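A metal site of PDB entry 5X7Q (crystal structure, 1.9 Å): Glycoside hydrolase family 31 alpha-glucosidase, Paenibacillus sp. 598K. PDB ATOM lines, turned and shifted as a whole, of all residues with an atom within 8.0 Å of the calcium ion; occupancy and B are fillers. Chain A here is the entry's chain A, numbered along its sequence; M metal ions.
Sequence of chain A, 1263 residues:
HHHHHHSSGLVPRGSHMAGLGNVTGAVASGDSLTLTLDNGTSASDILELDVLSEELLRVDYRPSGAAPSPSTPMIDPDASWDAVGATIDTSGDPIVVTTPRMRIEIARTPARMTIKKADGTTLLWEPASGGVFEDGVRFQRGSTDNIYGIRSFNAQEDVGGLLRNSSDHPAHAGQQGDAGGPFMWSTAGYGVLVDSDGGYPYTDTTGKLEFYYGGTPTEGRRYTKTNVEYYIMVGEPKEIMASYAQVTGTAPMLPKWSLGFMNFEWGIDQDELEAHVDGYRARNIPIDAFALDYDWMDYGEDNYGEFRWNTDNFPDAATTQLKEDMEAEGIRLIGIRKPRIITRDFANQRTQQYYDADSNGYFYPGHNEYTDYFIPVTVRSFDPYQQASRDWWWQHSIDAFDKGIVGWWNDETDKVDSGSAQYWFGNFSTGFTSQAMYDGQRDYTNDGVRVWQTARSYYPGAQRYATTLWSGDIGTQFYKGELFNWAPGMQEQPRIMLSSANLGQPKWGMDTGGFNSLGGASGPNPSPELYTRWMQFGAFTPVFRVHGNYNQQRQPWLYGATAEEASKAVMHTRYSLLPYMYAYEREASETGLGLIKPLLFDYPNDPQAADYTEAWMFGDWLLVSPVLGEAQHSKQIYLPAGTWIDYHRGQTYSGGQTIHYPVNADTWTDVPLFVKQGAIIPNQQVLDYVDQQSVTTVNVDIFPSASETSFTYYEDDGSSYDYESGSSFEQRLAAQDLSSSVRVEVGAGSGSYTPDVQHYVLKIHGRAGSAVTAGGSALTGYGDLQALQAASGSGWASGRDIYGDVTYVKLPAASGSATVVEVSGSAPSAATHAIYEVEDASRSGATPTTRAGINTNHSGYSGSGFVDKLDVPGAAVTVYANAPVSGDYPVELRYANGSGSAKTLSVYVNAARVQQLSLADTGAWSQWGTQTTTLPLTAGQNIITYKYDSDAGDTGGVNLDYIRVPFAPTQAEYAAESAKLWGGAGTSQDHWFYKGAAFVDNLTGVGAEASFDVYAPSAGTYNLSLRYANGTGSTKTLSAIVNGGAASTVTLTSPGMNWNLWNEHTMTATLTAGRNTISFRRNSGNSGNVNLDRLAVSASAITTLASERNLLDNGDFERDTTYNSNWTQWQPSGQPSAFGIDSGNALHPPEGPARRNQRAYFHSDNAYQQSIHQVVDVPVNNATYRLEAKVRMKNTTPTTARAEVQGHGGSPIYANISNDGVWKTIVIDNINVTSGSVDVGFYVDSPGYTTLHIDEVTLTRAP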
ATOM      1  N   GLN A 786     -23.587 -23.169  13.406  1.00  0.00           N
ATOM      2  CA  GLN A 786     -24.301 -21.964  13.842  1.00  0.00           C
ATOM      3  C   GLN A 786     -25.136 -22.199  15.108  1.00  0.00           C
ATOM      4  O   GLN A 786     -25.027 -21.438  16.070  1.00  0.00           O
ATOM      5  CB  GLN A 786     -25.214 -21.431  12.719  1.00  0.00           C
ATOM      6  CG  GLN A 786     -25.805 -20.052  13.008  1.00  0.00           C
ATOM      7  CD  GLN A 786     -27.319 -20.030  12.927  1.00  0.00           C
ATOM      8  OE1 GLN A 786     -27.901 -20.178  11.845  1.00  0.00           O
ATOM      9  NE2 GLN A 786     -27.980 -19.832  14.077  1.00  0.00           N
ATOM     10  N   ILE A 835     -21.760 -22.801   3.899  1.00  0.00           N
ATOM     11  CA  ILE A 835     -22.435 -21.510   4.140  1.00  0.00           C
ATOM     12  C   ILE A 835     -21.469 -20.511   4.757  1.00  0.00           C
ATOM     13  O   ILE A 835     -20.779 -20.829   5.726  1.00  0.00           O
ATOM     14  CB  ILE A 835     -23.738 -21.649   4.988  1.00  0.00           C
ATOM     15  CG1 ILE A 835     -24.408 -20.274   5.161  1.00  0.00           C
ATOM     16  CG2 ILE A 835     -23.489 -22.263   6.361  1.00  0.00           C
ATOM     17  CD1 ILE A 835     -25.855 -20.349   5.604  1.00  0.00           C
ATOM     18  N   TYR A 836     -21.397 -19.314   4.157  1.00  0.00           N
ATOM     19  CA  TYR A 836     -20.617 -18.214   4.685  1.00  0.00           C
ATOM     20  C   TYR A 836     -21.542 -17.076   5.096  1.00  0.00           C
ATOM     21  O   TYR A 836     -22.101 -16.393   4.246  1.00  0.00           O
ATOM     22  CB  TYR A 836     -19.628 -17.715   3.644  1.00  0.00           C
ATOM     23  CG  TYR A 836     -18.611 -18.732   3.230  1.00  0.00           C
ATOM     24  CD1 TYR A 836     -18.874 -19.636   2.213  1.00  0.00           C
ATOM     25  CD2 TYR A 836     -17.367 -18.789   3.849  1.00  0.00           C
ATOM     26  CE1 TYR A 836     -17.944 -20.585   1.828  1.00  0.00           C
ATOM     27  CE2 TYR A 836     -16.413 -19.735   3.479  1.00  0.00           C
ATOM     28  CZ  TYR A 836     -16.707 -20.619   2.468  1.00  0.00           C
ATOM     29  OH  TYR A 836     -15.776 -21.540   2.074  1.00  0.00           O
ATOM     30  N   GLU A 837     -21.700 -16.851   6.403  1.00  0.00           N
ATOM     31  CA  GLU A 837     -22.510 -15.720   6.875  1.00  0.00           C
ATOM     32  C   GLU A 837     -21.719 -14.434   6.649  1.00  0.00           C
ATOM     33  O   GLU A 837     -20.620 -14.287   7.182  1.00  0.00           O
ATOM     34  CB  GLU A 837     -22.852 -15.884   8.360  1.00  0.00           C
ATOM     35  CG  GLU A 837     -23.704 -17.101   8.693  1.00  0.00           C
ATOM     36  CD  GLU A 837     -25.157 -17.018   8.228  1.00  0.00           C
ATOM     37  OE1 GLU A 837     -25.641 -15.933   7.848  1.00  0.00           O
ATOM     38  OE2 GLU A 837     -25.819 -18.060   8.268  1.00  0.00           O
ATOM     39  N   VAL A 838     -22.262 -13.514   5.851  1.00  0.00           N
ATOM     40  CA  VAL A 838     -21.487 -12.334   5.447  1.00  0.00           C
ATOM     41  C   VAL A 838     -21.225 -11.336   6.564  1.00  0.00           C
ATOM     42  O   VAL A 838     -20.278 -10.566   6.485  1.00  0.00           O
ATOM     43  CB  VAL A 838     -22.043 -11.644   4.186  1.00  0.00           C
ATOM     44  CG1 VAL A 838     -21.839 -12.563   2.988  1.00  0.00           C
ATOM     45  CG2 VAL A 838     -23.507 -11.241   4.362  1.00  0.00           C
ATOM     46  N   GLU A 839     -22.027 -11.386   7.638  1.00  0.00           N
ATOM     47  CA  GLU A 839     -21.719 -10.588   8.839  1.00  0.00           C
ATOM     48  C   GLU A 839     -20.408 -11.018   9.523  1.00  0.00           C
ATOM     49  O   GLU A 839     -19.837 -10.222  10.258  1.00  0.00           O
ATOM     50  CB  GLU A 839     -22.877 -10.602   9.855  1.00  0.00           C
ATOM     51  CG  GLU A 839     -23.215 -11.951  10.475  1.00  0.00           C
ATOM     52  CD  GLU A 839     -24.188 -12.781   9.664  1.00  0.00           C
ATOM     53  OE1 GLU A 839     -24.351 -12.574   8.443  1.00  0.00           O
ATOM     54  OE2 GLU A 839     -24.803 -13.688  10.244  1.00  0.00           O
ATOM     55  N   ASP A 840     -19.951 -12.248   9.278  1.00  0.00           N
ATOM     56  CA  ASP A 840     -18.616 -12.707   9.703  1.00  0.00           C
ATOM     57  C   ASP A 840     -17.496 -12.382   8.711  1.00  0.00           C
ATOM     58  O   ASP A 840     -16.341 -12.660   9.013  1.00  0.00           O
ATOM     59  CB  ASP A 840     -18.599 -14.219   9.912  1.00  0.00           C
ATOM     60  CG  ASP A 840     -19.640 -14.690  10.921  1.00  0.00           C
ATOM     61  OD1 ASP A 840     -20.103 -13.850  11.704  1.00  0.00           O
ATOM     62  OD2 ASP A 840     -19.998 -15.893  10.888  1.00  0.00           O
ATOM     63  N   ASN A 855     -25.913  -5.687  11.005  1.00  0.00           N
ATOM     64  CA  ASN A 855     -27.164  -5.318  11.672  1.00  0.00           C
ATOM     65  C   ASN A 855     -28.076  -6.528  11.939  1.00  0.00           C
ATOM     66  O   ASN A 855     -27.856  -7.632  11.425  1.00  0.00           O
ATOM     67  CB  ASN A 855     -27.896  -4.233  10.866  1.00  0.00           C
ATOM     68  CG  ASN A 855     -28.562  -3.195  11.752  1.00  0.00           C
ATOM     69  OD1 ASN A 855     -29.052  -3.517  12.836  1.00  0.00           O
ATOM     70  ND2 ASN A 855     -28.599  -1.951  11.287  1.00  0.00           N
ATOM     71  N   GLY A 860     -35.708 -12.532  10.085  1.00  0.00           N
ATOM     72  CA  GLY A 860     -35.643 -13.562   9.044  1.00  0.00           C
ATOM     73  C   GLY A 860     -34.240 -13.932   8.552  1.00  0.00           C
ATOM     74  O   GLY A 860     -34.108 -14.722   7.614  1.00  0.00           O
ATOM     75  N   TYR A 861     -33.214 -13.374   9.181  1.00  0.00           N
ATOM     76  CA  TYR A 861     -31.831 -13.601   8.780  1.00  0.00           C
ATOM     77  C   TYR A 861     -31.313 -14.884   9.412  1.00  0.00           C
ATOM     78  O   TYR A 861     -31.734 -15.267  10.509  1.00  0.00           O
ATOM     79  CB  TYR A 861     -30.930 -12.413   9.172  1.00  0.00           C
ATOM     80  CG  TYR A 861     -30.942 -12.079  10.663  1.00  0.00           C
ATOM     81  CD1 TYR A 861     -30.144 -12.772  11.564  1.00  0.00           C
ATOM     82  CD2 TYR A 861     -31.747 -11.057  11.141  1.00  0.00           C
ATOM     83  CE1 TYR A 861     -30.174 -12.464  12.928  1.00  0.00           C
ATOM     84  CE2 TYR A 861     -31.795 -10.729  12.489  1.00  0.00           C
ATOM     85  CZ  TYR A 861     -31.004 -11.430  13.376  1.00  0.00           C
ATOM     86  OH  TYR A 861     -31.035 -11.106  14.711  1.00  0.00           O
ATOM     87  N   SER A 862     -30.416 -15.549   8.684  1.00  0.00           N
ATOM     88  CA  SER A 862     -29.587 -16.655   9.218  1.00  0.00           C
ATOM     89  C   SER A 862     -28.384 -16.141  10.033  1.00  0.00           C
ATOM     90  O   SER A 862     -27.926 -15.008   9.867  1.00  0.00           O
ATOM     91  CB  SER A 862     -29.106 -17.522   8.048  1.00  0.00           C
ATOM     92  OG  SER A 862     -28.285 -18.576   8.487  1.00  0.00           O
ATOM     93  N   GLY A 863     -27.881 -16.985  10.931  1.00  0.00           N
ATOM     94  CA  GLY A 863     -26.750 -16.629  11.780  1.00  0.00           C
ATOM     95  C   GLY A 863     -27.063 -15.504  12.751  1.00  0.00           C
ATOM     96  O   GLY A 863     -28.212 -15.357  13.185  1.00  0.00           O
ATOM     97  N   SER A 864     -26.062 -14.699  13.061  1.00  0.00           N
ATOM     98  CA  SER A 864     -26.174 -13.647  14.064  1.00  0.00           C
ATOM     99  C   SER A 864     -26.612 -12.317  13.482  1.00  0.00           C
ATOM    100  O   SER A 864     -26.829 -11.362  14.231  1.00  0.00           O
ATOM    101  CB  SER A 864     -24.847 -13.495  14.810  1.00  0.00           C
ATOM    102  OG  SER A 864     -23.803 -13.144  13.920  1.00  0.00           O
ATOM    103  N   GLY A 865     -26.762 -12.230  12.161  1.00  0.00           N
ATOM    104  CA  GLY A 865     -27.198 -10.978  11.541  1.00  0.00           C
ATOM    105  C   GLY A 865     -27.105 -10.955  10.019  1.00  0.00           C
ATOM    106  O   GLY A 865     -27.162 -11.977   9.363  1.00  0.00           O
ATOM    107  N   PHE A 866     -26.991  -9.744   9.484  1.00  0.00           N
ATOM    108  CA  PHE A 866     -26.786  -9.546   8.049  1.00  0.00           C
ATOM    109  C   PHE A 866     -25.949  -8.297   7.813  1.00  0.00           C
ATOM    110  O   PHE A 866     -25.674  -7.541   8.753  1.00  0.00           O
ATOM    111  CB  PHE A 866     -28.132  -9.407   7.344  1.00  0.00           C
ATOM    112  CG  PHE A 866     -29.012  -8.330   7.915  1.00  0.00           C
ATOM    113  CD1 PHE A 866     -28.939  -7.028   7.423  1.00  0.00           C
ATOM    114  CD2 PHE A 866     -29.914  -8.628   8.927  1.00  0.00           C
ATOM    115  CE1 PHE A 866     -29.764  -6.029   7.951  1.00  0.00           C
ATOM    116  CE2 PHE A 866     -30.741  -7.642   9.449  1.00  0.00           C
ATOM    117  CZ  PHE A 866     -30.661  -6.333   8.956  1.00  0.00           C
ATOM    118  N   VAL A 867     -25.562  -8.072   6.567  1.00  0.00           N
ATOM    119  CA  VAL A 867     -24.750  -6.932   6.208  1.00  0.00           C
ATOM    120  C   VAL A 867     -25.636  -5.868   5.561  1.00  0.00           C
ATOM    121  O   VAL A 867     -26.372  -6.171   4.617  1.00  0.00           O
ATOM    122  CB  VAL A 867     -23.575  -7.325   5.278  1.00  0.00           C
ATOM    123  CG1 VAL A 867     -22.908  -6.088   4.668  1.00  0.00           C
ATOM    124  CG2 VAL A 867     -22.560  -8.157   6.051  1.00  0.00           C
ATOM    125  N   ARG A 894     -27.980 -14.942  -0.539  1.00  0.00           N
ATOM    126  CA  ARG A 894     -29.233 -14.630   0.145  1.00  0.00           C
ATOM    127  C   ARG A 894     -29.247 -13.145   0.491  1.00  0.00           C
ATOM    128  O   ARG A 894     -28.297 -12.636   1.120  1.00  0.00           O
ATOM    129  CB  ARG A 894     -29.439 -15.473   1.402  1.00  0.00           C
ATOM    130  CG  ARG A 894     -30.853 -15.314   1.990  1.00  0.00           C
ATOM    131  CD  ARG A 894     -31.261 -16.508   2.833  1.00  0.00           C
ATOM    132  NE  ARG A 894     -32.682 -16.582   3.220  1.00  0.00           N
ATOM    133  CZ  ARG A 894     -33.212 -16.125   4.368  1.00  0.00           C
ATOM    134  NH1 ARG A 894     -32.492 -15.475   5.279  1.00  0.00           N
ATOM    135  NH2 ARG A 894     -34.518 -16.301   4.580  1.00  0.00           N
ATOM    136  N   TRP A 928     -36.679 -12.302   2.479  1.00  0.00           N
ATOM    137  CA  TRP A 928     -35.384 -12.644   1.897  1.00  0.00           C
ATOM    138  C   TRP A 928     -35.563 -13.510   0.669  1.00  0.00           C
ATOM    139  O   TRP A 928     -36.489 -14.321   0.602  1.00  0.00           O
ATOM    140  CB  TRP A 928     -34.516 -13.367   2.936  1.00  0.00           C
ATOM    141  CG  TRP A 928     -34.301 -12.526   4.167  1.00  0.00           C
ATOM    142  CD1 TRP A 928     -35.157 -12.397   5.229  1.00  0.00           C
ATOM    143  CD2 TRP A 928     -33.169 -11.672   4.458  1.00  0.00           C
ATOM    144  NE1 TRP A 928     -34.632 -11.531   6.157  1.00  0.00           N
ATOM    145  CE2 TRP A 928     -33.412 -11.069   5.714  1.00  0.00           C
ATOM    146  CE3 TRP A 928     -31.985 -11.368   3.774  1.00  0.00           C
ATOM    147  CZ2 TRP A 928     -32.510 -10.178   6.314  1.00  0.00           C
ATOM    148  CZ3 TRP A 928     -31.093 -10.467   4.358  1.00  0.00           C
ATOM    149  CH2 TRP A 928     -31.358  -9.884   5.629  1.00  0.00           C
ATOM    150  N   LEU A 960     -27.457  -8.223   2.748  1.00  0.00           N
ATOM    151  CA  LEU A 960     -26.948  -9.542   2.361  1.00  0.00           C
ATOM    152  C   LEU A 960     -26.816 -10.387   3.601  1.00  0.00           C
ATOM    153  O   LEU A 960     -26.345  -9.922   4.648  1.00  0.00           O
ATOM    154  CB  LEU A 960     -25.595  -9.411   1.664  1.00  0.00           C
ATOM    155  CG  LEU A 960     -25.454  -8.480   0.464  1.00  0.00           C
ATOM    156  CD1 LEU A 960     -24.035  -8.555  -0.100  1.00  0.00           C
ATOM    157  CD2 LEU A 960     -26.473  -8.785  -0.632  1.00  0.00           C
ATOM    158  N   ASP A 961     -27.262 -11.627   3.503  1.00  0.00           N
ATOM    159  CA  ASP A 961     -27.357 -12.490   4.680  1.00  0.00           C
ATOM    160  C   ASP A 961     -26.249 -13.541   4.696  1.00  0.00           C
ATOM    161  O   ASP A 961     -25.581 -13.729   5.735  1.00  0.00           O
ATOM    162  CB  ASP A 961     -28.713 -13.196   4.699  1.00  0.00           C
ATOM    163  CG  ASP A 961     -28.981 -13.909   6.010  1.00  0.00           C
ATOM    164  OD1 ASP A 961     -28.238 -13.718   7.010  1.00  0.00           O
ATOM    165  OD2 ASP A 961     -29.960 -14.675   6.032  1.00  0.00           O
ATOM    166  N   TYR A 962     -26.089 -14.244   3.584  1.00  0.00           N
ATOM    167  CA  TYR A 962     -25.002 -15.216   3.411  1.00  0.00           C
ATOM    168  C   TYR A 962     -24.803 -15.578   1.963  1.00  0.00           C
ATOM    169  O   TYR A 962     -25.610 -15.203   1.115  1.00  0.00           O
ATOM    170  CB  TYR A 962     -25.261 -16.516   4.215  1.00  0.00           C
ATOM    171  CG  TYR A 962     -26.536 -17.257   3.857  1.00  0.00           C
ATOM    172  CD1 TYR A 962     -26.652 -17.968   2.651  1.00  0.00           C
ATOM    173  CD2 TYR A 962     -27.614 -17.286   4.735  1.00  0.00           C
ATOM    174  CE1 TYR A 962     -27.812 -18.658   2.336  1.00  0.00           C
ATOM    175  CE2 TYR A 962     -28.779 -18.000   4.422  1.00  0.00           C
ATOM    176  CZ  TYR A 962     -28.858 -18.677   3.229  1.00  0.00           C
ATOM    177  OH  TYR A 962     -30.010 -19.361   2.915  1.00  0.00           O
ATOM    178  N   ILE A 963     -23.725 -16.317   1.693  1.00  0.00           N
ATOM    179  CA  ILE A 963     -23.596 -17.032   0.431  1.00  0.00           C
ATOM    180  C   ILE A 963     -23.398 -18.519   0.709  1.00  0.00           C
ATOM    181  O   ILE A 963     -22.886 -18.892   1.774  1.00  0.00           O
ATOM    182  CB  ILE A 963     -22.466 -16.493  -0.494  1.00  0.00           C
ATOM    183  CG1 ILE A 963     -21.070 -16.719   0.112  1.00  0.00           C
ATOM    184  CG2 ILE A 963     -22.701 -15.011  -0.779  1.00  0.00           C
ATOM    185  CD1 ILE A 963     -19.935 -16.396  -0.837  1.00  0.00           C
HETATM  186 CA    CA M   1     -26.398 -13.951   8.213  1.00  0.00          CA
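The side-chain carboxylate (OD2) of Asp 961 lies within salt-bridge range of the guanidinium group (NH1) of Arg 894, at 2.8 Å.
O of Asp 961 sits close to N of Val 838 (3.3 Å).
The side-chain carboxylate (OE2) of Glu 839 sits close to the backbone NH (N) of Ser 864 (3.2 Å).
The calcium ion is bound by the side-chain carboxylate (OE1) of Glu 837, the side-chain carboxylate (OD1) of Asp 961, the backbone carbonyl oxygen (O) of Gly 865, the side-chain carboxylate (OE1) of Glu 839, the backbone carbonyl oxygen (O) of Ser 862, the side-chain carboxylate (OE2) of Glu 839 and the backbone carbonyl oxygen (O) of Asp 961.
Along chain A the residues within 4 Å of the calcium ion span positions 837 to 961.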
